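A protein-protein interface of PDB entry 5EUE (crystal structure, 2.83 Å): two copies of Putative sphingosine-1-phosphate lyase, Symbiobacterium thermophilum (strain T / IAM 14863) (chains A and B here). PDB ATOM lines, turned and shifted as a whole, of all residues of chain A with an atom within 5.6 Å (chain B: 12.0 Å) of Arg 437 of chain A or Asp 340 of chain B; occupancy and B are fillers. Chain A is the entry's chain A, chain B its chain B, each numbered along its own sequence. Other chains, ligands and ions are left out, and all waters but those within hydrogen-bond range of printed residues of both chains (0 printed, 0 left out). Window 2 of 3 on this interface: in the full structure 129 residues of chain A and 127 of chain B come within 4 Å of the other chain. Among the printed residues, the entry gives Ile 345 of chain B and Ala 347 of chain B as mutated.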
ATOM      1  N   VAL A 199       1.622  25.652   7.434  1.00  0.00           N
ATOM      2  CA  VAL A 199       0.389  25.247   6.717  1.00  0.00           C
ATOM      3  C   VAL A 199       0.084  26.180   5.541  1.00  0.00           C
ATOM      4  O   VAL A 199      -0.381  25.728   4.501  1.00  0.00           O
ATOM      5  CB  VAL A 199      -0.859  25.046   7.617  1.00  0.00           C
ATOM      6  CG1 VAL A 199      -0.758  23.767   8.420  1.00  0.00           C
ATOM      7  CG2 VAL A 199      -1.095  26.231   8.532  1.00  0.00           C
ATOM      8  N   HIS A 252      -3.233  34.215   2.787  1.00  0.00           N
ATOM      9  CA  HIS A 252      -3.639  35.447   3.468  1.00  0.00           C
ATOM     10  C   HIS A 252      -2.696  36.645   3.281  1.00  0.00           C
ATOM     11  O   HIS A 252      -2.998  37.721   3.808  1.00  0.00           O
ATOM     12  CB  HIS A 252      -3.889  35.154   4.966  1.00  0.00           C
ATOM     13  CG  HIS A 252      -4.591  33.842   5.179  1.00  0.00           C
ATOM     14  ND1 HIS A 252      -4.021  32.837   5.936  1.00  0.00           N
ATOM     15  CD2 HIS A 252      -5.733  33.374   4.619  1.00  0.00           C
ATOM     16  CE1 HIS A 252      -4.841  31.800   5.827  1.00  0.00           C
ATOM     17  NE2 HIS A 252      -5.889  32.084   5.051  1.00  0.00           N
ATOM     18  N   TYR A 419     -18.620  32.382   1.170  1.00  0.00           N
ATOM     19  CA  TYR A 419     -18.701  31.748  -0.144  1.00  0.00           C
ATOM     20  C   TYR A 419     -19.824  32.353  -0.927  1.00  0.00           C
ATOM     21  O   TYR A 419     -19.628  32.674  -2.092  1.00  0.00           O
ATOM     22  CB  TYR A 419     -18.854  30.225  -0.048  1.00  0.00           C
ATOM     23  CG  TYR A 419     -17.659  29.502   0.537  1.00  0.00           C
ATOM     24  CD1 TYR A 419     -16.359  29.924   0.266  1.00  0.00           C
ATOM     25  CD2 TYR A 419     -17.823  28.353   1.305  1.00  0.00           C
ATOM     26  CE1 TYR A 419     -15.253  29.229   0.760  1.00  0.00           C
ATOM     27  CE2 TYR A 419     -16.722  27.642   1.792  1.00  0.00           C
ATOM     28  CZ  TYR A 419     -15.439  28.084   1.516  1.00  0.00           C
ATOM     29  OH  TYR A 419     -14.363  27.386   1.998  1.00  0.00           O
ATOM     30  N   LEU A 435     -10.957  30.345  -0.896  1.00  0.00           N
ATOM     31  CA  LEU A 435     -10.081  29.800   0.145  1.00  0.00           C
ATOM     32  C   LEU A 435     -10.866  28.942   1.156  1.00  0.00           C
ATOM     33  O   LEU A 435     -12.066  29.152   1.370  1.00  0.00           O
ATOM     34  CB  LEU A 435      -9.381  30.953   0.924  1.00  0.00           C
ATOM     35  CG  LEU A 435      -8.629  32.022   0.150  1.00  0.00           C
ATOM     36  CD1 LEU A 435      -8.240  33.170   1.062  1.00  0.00           C
ATOM     37  CD2 LEU A 435      -7.383  31.471  -0.488  1.00  0.00           C
ATOM     38  N   HIS A 436     -10.166  28.006   1.803  1.00  0.00           N
ATOM     39  CA  HIS A 436     -10.715  27.206   2.891  1.00  0.00           C
ATOM     40  C   HIS A 436      -9.706  27.109   4.052  1.00  0.00           C
ATOM     41  O   HIS A 436      -8.618  27.690   3.965  1.00  0.00           O
ATOM     42  CB  HIS A 436     -11.266  25.841   2.427  1.00  0.00           C
ATOM     43  CG  HIS A 436     -10.272  24.895   1.829  1.00  0.00           C
ATOM     44  ND1 HIS A 436     -10.680  23.683   1.293  1.00  0.00           N
ATOM     45  CD2 HIS A 436      -8.934  25.008   1.677  1.00  0.00           C
ATOM     46  CE1 HIS A 436      -9.585  23.102   0.842  1.00  0.00           C
ATOM     47  NE2 HIS A 436      -8.509  23.862   1.050  1.00  0.00           N
ATOM     48  N   ARG A 437     -10.112  26.484   5.168  1.00  0.00           N
ATOM     49  CA  ARG A 437      -9.282  26.295   6.361  1.00  0.00           C
ATOM     50  C   ARG A 437      -8.578  27.586   6.833  1.00  0.00           C
ATOM     51  O   ARG A 437      -7.342  27.590   6.854  1.00  0.00           O
ATOM     52  CB  ARG A 437      -8.252  25.154   6.127  1.00  0.00           C
ATOM     53  CG  ARG A 437      -8.868  23.762   5.964  1.00  0.00           C
ATOM     54  CD  ARG A 437      -7.968  22.835   5.172  1.00  0.00           C
ATOM     55  NE  ARG A 437      -7.911  21.490   5.753  1.00  0.00           N
ATOM     56  CZ  ARG A 437      -8.654  20.455   5.363  1.00  0.00           C
ATOM     57  NH1 ARG A 437      -9.518  20.586   4.360  1.00  0.00           N
ATOM     58  NH2 ARG A 437      -8.531  19.279   5.963  1.00  0.00           N
ATOM     59  N   PRO A 438      -9.271  28.710   7.166  1.00  0.00           N
ATOM     60  CA  PRO A 438     -10.732  28.942   7.249  1.00  0.00           C
ATOM     61  C   PRO A 438     -11.426  29.339   5.945  1.00  0.00           C
ATOM     62  O   PRO A 438     -10.765  29.832   5.024  1.00  0.00           O
ATOM     63  CB  PRO A 438     -10.830  30.095   8.258  1.00  0.00           C
ATOM     64  CG  PRO A 438      -9.587  30.906   8.008  1.00  0.00           C
ATOM     65  CD  PRO A 438      -8.516  29.902   7.625  1.00  0.00           C
ATOM     66  N   PRO A 439     -12.776  29.194   5.857  1.00  0.00           N
ATOM     67  CA  PRO A 439     -13.471  29.623   4.640  1.00  0.00           C
ATOM     68  C   PRO A 439     -13.393  31.144   4.514  1.00  0.00           C
ATOM     69  O   PRO A 439     -13.881  31.897   5.377  1.00  0.00           O
ATOM     70  CB  PRO A 439     -14.908  29.132   4.859  1.00  0.00           C
ATOM     71  CG  PRO A 439     -14.821  28.138   5.959  1.00  0.00           C
ATOM     72  CD  PRO A 439     -13.742  28.653   6.836  1.00  0.00           C
ATOM     73  N   ALA A 486     -16.952  21.264  -0.518  1.00  0.00           N
ATOM     74  CA  ALA A 486     -15.503  21.079  -0.628  1.00  0.00           C
ATOM     75  C   ALA A 486     -14.749  21.372   0.672  1.00  0.00           C
ATOM     76  O   ALA A 486     -13.811  20.640   0.988  1.00  0.00           O
ATOM     77  CB  ALA A 486     -14.958  21.948  -1.750  1.00  0.00           C
ATOM     78  N   ALA A 487     -15.141  22.448   1.410  1.00  0.00           N
ATOM     79  CA  ALA A 487     -14.507  22.856   2.674  1.00  0.00           C
ATOM     80  C   ALA A 487     -14.575  21.742   3.729  1.00  0.00           C
ATOM     81  O   ALA A 487     -13.611  21.566   4.484  1.00  0.00           O
ATOM     82  CB  ALA A 487     -15.127  24.141   3.203  1.00  0.00           C
ATOM     83  N   PRO A 491     -10.775  13.780   1.749  1.00  0.00           N
ATOM     84  CA  PRO A 491      -9.806  14.139   0.694  1.00  0.00           C
ATOM     85  C   PRO A 491      -9.982  13.381  -0.618  1.00  0.00           C
ATOM     86  O   PRO A 491      -9.692  13.946  -1.668  1.00  0.00           O
ATOM     87  CB  PRO A 491      -8.445  13.892   1.351  1.00  0.00           C
ATOM     88  CG  PRO A 491      -8.707  13.968   2.808  1.00  0.00           C
ATOM     89  CD  PRO A 491     -10.078  13.394   2.995  1.00  0.00           C
ATOM     90  N   PHE B 336      -1.586  16.318  -9.916  1.00  0.00           N
ATOM     91  CA  PHE B 336      -1.238  16.666  -8.538  1.00  0.00           C
ATOM     92  C   PHE B 336      -2.453  17.286  -7.921  1.00  0.00           C
ATOM     93  O   PHE B 336      -2.991  18.249  -8.474  1.00  0.00           O
ATOM     94  CB  PHE B 336      -0.087  17.679  -8.441  1.00  0.00           C
ATOM     95  CG  PHE B 336       0.008  18.296  -7.055  1.00  0.00           C
ATOM     96  CD1 PHE B 336       0.519  17.565  -5.981  1.00  0.00           C
ATOM     97  CD2 PHE B 336      -0.461  19.586  -6.812  1.00  0.00           C
ATOM     98  CE1 PHE B 336       0.580  18.123  -4.696  1.00  0.00           C
ATOM     99  CE2 PHE B 336      -0.413  20.135  -5.527  1.00  0.00           C
ATOM    100  CZ  PHE B 336       0.118  19.406  -4.478  1.00  0.00           C
ATOM    101  N   ILE B 337      -2.869  16.775  -6.760  1.00  0.00           N
ATOM    102  CA  ILE B 337      -4.026  17.328  -6.052  1.00  0.00           C
ATOM    103  C   ILE B 337      -3.697  17.587  -4.574  1.00  0.00           C
ATOM    104  O   ILE B 337      -3.167  16.700  -3.901  1.00  0.00           O
ATOM    105  CB  ILE B 337      -5.322  16.497  -6.252  1.00  0.00           C
ATOM    106  CG1 ILE B 337      -5.519  16.100  -7.732  1.00  0.00           C
ATOM    107  CG2 ILE B 337      -6.530  17.301  -5.760  1.00  0.00           C
ATOM    108  CD1 ILE B 337      -6.384  14.877  -7.957  1.00  0.00           C
ATOM    109  N   ALA B 338      -3.971  18.823  -4.102  1.00  0.00           N
ATOM    110  CA  ALA B 338      -3.797  19.283  -2.718  1.00  0.00           C
ATOM    111  C   ALA B 338      -5.191  19.624  -2.176  1.00  0.00           C
ATOM    112  O   ALA B 338      -5.948  20.367  -2.826  1.00  0.00           O
ATOM    113  CB  ALA B 338      -2.902  20.499  -2.672  1.00  0.00           C
ATOM    114  N   ALA B 339      -5.552  19.042  -1.006  1.00  0.00           N
ATOM    115  CA  ALA B 339      -6.888  19.225  -0.428  1.00  0.00           C
ATOM    116  C   ALA B 339      -6.937  20.045   0.837  1.00  0.00           C
ATOM    117  O   ALA B 339      -7.961  20.686   1.072  1.00  0.00           O
ATOM    118  CB  ALA B 339      -7.554  17.880  -0.191  1.00  0.00           C
ATOM    119  N   ASP B 340      -5.875  20.014   1.669  1.00  0.00           N
ATOM    120  CA  ASP B 340      -5.869  20.720   2.963  1.00  0.00           C
ATOM    121  C   ASP B 340      -5.102  22.077   2.966  1.00  0.00           C
ATOM    122  O   ASP B 340      -4.752  22.587   4.044  1.00  0.00           O
ATOM    123  CB  ASP B 340      -5.339  19.784   4.073  1.00  0.00           C
ATOM    124  CG  ASP B 340      -5.845  18.345   4.048  1.00  0.00           C
ATOM    125  OD1 ASP B 340      -7.067  18.143   3.891  1.00  0.00           O
ATOM    126  OD2 ASP B 340      -5.023  17.426   4.225  1.00  0.00           O
ATOM    127  N   TRP B 341      -4.861  22.670   1.765  1.00  0.00           N
ATOM    128  CA  TRP B 341      -4.091  23.910   1.662  1.00  0.00           C
ATOM    129  C   TRP B 341      -4.949  25.171   1.910  1.00  0.00           C
ATOM    130  O   TRP B 341      -5.884  25.425   1.156  1.00  0.00           O
ATOM    131  CB  TRP B 341      -3.308  23.974   0.327  1.00  0.00           C
ATOM    132  CG  TRP B 341      -2.439  25.189   0.179  1.00  0.00           C
ATOM    133  CD1 TRP B 341      -1.581  25.706   1.107  1.00  0.00           C
ATOM    134  CD2 TRP B 341      -2.366  26.056  -0.964  1.00  0.00           C
ATOM    135  NE1 TRP B 341      -1.010  26.865   0.634  1.00  0.00           N
ATOM    136  CE2 TRP B 341      -1.443  27.084  -0.652  1.00  0.00           C
ATOM    137  CE3 TRP B 341      -3.021  26.090  -2.210  1.00  0.00           C
ATOM    138  CZ2 TRP B 341      -1.113  28.098  -1.565  1.00  0.00           C
ATOM    139  CZ3 TRP B 341      -2.705  27.107  -3.103  1.00  0.00           C
ATOM    140  CH2 TRP B 341      -1.763  28.096  -2.776  1.00  0.00           C
ATOM    141  N   PRO B 342      -4.637  25.995   2.937  1.00  0.00           N
ATOM    142  CA  PRO B 342      -5.443  27.207   3.190  1.00  0.00           C
ATOM    143  C   PRO B 342      -5.736  28.082   1.969  1.00  0.00           C
ATOM    144  O   PRO B 342      -6.760  28.753   1.959  1.00  0.00           O
ATOM    145  CB  PRO B 342      -4.628  27.955   4.238  1.00  0.00           C
ATOM    146  CG  PRO B 342      -3.907  26.904   4.962  1.00  0.00           C
ATOM    147  CD  PRO B 342      -3.573  25.846   3.954  1.00  0.00           C
ATOM    148  N   GLY B 343      -4.880  28.011   0.940  1.00  0.00           N
ATOM    149  CA  GLY B 343      -5.011  28.735  -0.324  1.00  0.00           C
ATOM    150  C   GLY B 343      -6.079  28.199  -1.259  1.00  0.00           C
ATOM    151  O   GLY B 343      -6.228  28.668  -2.392  1.00  0.00           O
ATOM    152  N   GLY B 344      -6.839  27.229  -0.773  1.00  0.00           N
ATOM    153  CA  GLY B 344      -7.911  26.584  -1.524  1.00  0.00           C
ATOM    154  C   GLY B 344      -7.521  25.229  -2.078  1.00  0.00           C
ATOM    155  O   GLY B 344      -6.472  24.678  -1.731  1.00  0.00           O
ATOM    156  N   ILE B 345      -8.391  24.680  -2.930  1.00  0.00           N
ATOM    157  CA  ILE B 345      -8.159  23.400  -3.594  1.00  0.00           C
ATOM    158  C   ILE B 345      -7.259  23.672  -4.791  1.00  0.00           C
ATOM    159  O   ILE B 345      -7.563  24.526  -5.617  1.00  0.00           O
ATOM    160  CB  ILE B 345      -9.489  22.698  -3.967  1.00  0.00           C
ATOM    161  CG1 ILE B 345     -10.270  22.330  -2.692  1.00  0.00           C
ATOM    162  CG2 ILE B 345      -9.253  21.459  -4.849  1.00  0.00           C
ATOM    163  CD1 ILE B 345     -11.741  22.153  -2.902  1.00  0.00           C
ATOM    164  N   TYR B 346      -6.126  22.985  -4.839  1.00  0.00           N
ATOM    165  CA  TYR B 346      -5.150  23.131  -5.903  1.00  0.00           C
ATOM    166  C   TYR B 346      -4.995  21.824  -6.619  1.00  0.00           C
ATOM    167  O   TYR B 346      -4.816  20.779  -5.995  1.00  0.00           O
ATOM    168  CB  TYR B 346      -3.800  23.567  -5.328  1.00  0.00           C
ATOM    169  CG  TYR B 346      -2.869  24.221  -6.324  1.00  0.00           C
ATOM    170  CD1 TYR B 346      -3.085  25.524  -6.759  1.00  0.00           C
ATOM    171  CD2 TYR B 346      -1.709  23.577  -6.748  1.00  0.00           C
ATOM    172  CE1 TYR B 346      -2.191  26.159  -7.617  1.00  0.00           C
ATOM    173  CE2 TYR B 346      -0.795  24.211  -7.587  1.00  0.00           C
ATOM    174  CZ  TYR B 346      -1.043  25.501  -8.026  1.00  0.00           C
ATOM    175  OH  TYR B 346      -0.157  26.139  -8.866  1.00  0.00           O
ATOM    176  N   ALA B 347      -5.077  21.898  -7.935  1.00  0.00           N
ATOM    177  CA  ALA B 347      -4.928  20.787  -8.856  1.00  0.00           C
ATOM    178  C   ALA B 347      -4.003  21.230  -9.977  1.00  0.00           C
ATOM    179  O   ALA B 347      -4.069  22.394 -10.398  1.00  0.00           O
ATOM    180  CB  ALA B 347      -6.281  20.418  -9.428  1.00  0.00           C
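O of Ala 339 of chain B lies close to NE2 of His 436 of chain A, 3.2 Å away. A ring nitrogen (NE2) of His 436 of chain A sits at hydrogen-bond distance from the backbone carbonyl oxygen (O) of Trp 341 of chain B. N of His 436 of chain A is in hydrogen-bond range of O of Pro 342 of chain B, 3.5 Å away. The guanidinium group of Arg 437 of chain A lies within salt-bridge range of the side-chain carboxylate of Asp 340 of chain B (2.8 Å).
OH of Tyr 419 of chain A lies within hydrogen-bond range of O of Leu 435 of chain A (3.0 Å).
Among the printed residues, pairs that only touch across the chains: Val 199 of chain A with Trp 341 of chain B, Val 199 of chain A with Pro 342 of chain B, Leu 435 of chain A with Pro 342 of chain B, Leu 435 of chain A with Gly 343 of chain B, His 436 of chain A with Gly 344 of chain B, His 436 of chain A with Ile 345 of chain B, Arg 437 of chain A with Ala 339 of chain B, Arg 437 of chain A with Pro 342 of chain B and Ala 486 of chain A with Ile 345 of chain B.
Val 199 of chain A touches just these residues of chain B: Trp 341 and Pro 342. Of the printed residues of chain B, Leu 435 of chain A touches Pro 342 (3.6 Å) and Gly 343 (3.6 Å). Of chain B, only Ala 339 (3.6 Å), Asp 340 (2.8 Å) and Pro 342 (3.8 Å) come within 4 Å of Arg 437 of chain A. No residue of chain B comes within 4 Å of Pro 438 of chain A. No residue of chain B comes within 4 Å of Pro 439 of chain A. No residue of chain B comes within 4 Å of Ala 487 of chain A. No residue of chain B comes within 4 Å of Pro 491 of chain A. Of the printed residues of chain A, Ala 339 of chain B touches His 436 and Arg 437. Asp 340 of chain B touches just one residue of chain A: Arg 437. Printed residues of chain A within 4 Å of Trp 341 of chain B: Val 199 (3.6 Å) and His 436 (3.1 Å). Of the printed residues of chain A, Gly 344 of chain B touches His 436 (3.5 Å). Printed residues of chain A within 4 Å of Ile 345 of chain B: His 436 and Ala 486. The nearest residue of chain A that does not touch Asp 340 of chain B is His 436 of chain A (4.3 Å). The nearest printed residue of chain A that does not touch Pro 342 of chain B is His 252 of chain A (4.2 Å).
Printed residues of chain A that touch a printed residue of chain B: Val 199, Leu 435, His 436, Arg 437 and Ala 486. Along chain A the printed residues that touch a printed residue of chain B span positions 199 to 486. Of the 12 printed residues of chain B, 7 touch a printed residue of chain A. Printed residues of chain B that touch a printed residue of chain A: Ala 339, Asp 340, Trp 341, Pro 342, Gly 343, Gly 344 and Ile 345. Hydrophobic or aromatic side chains of chain B within 4 Å of the printed part of chain A: Trp 341, Pro 342 and Ile 345. Among the printed residues, 13 pairs touch across the chains.
No position is printed for both chains. Of the 13 pairs that touch across the chains among the printed residues, none has its exchanged pair printed and touching as well.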
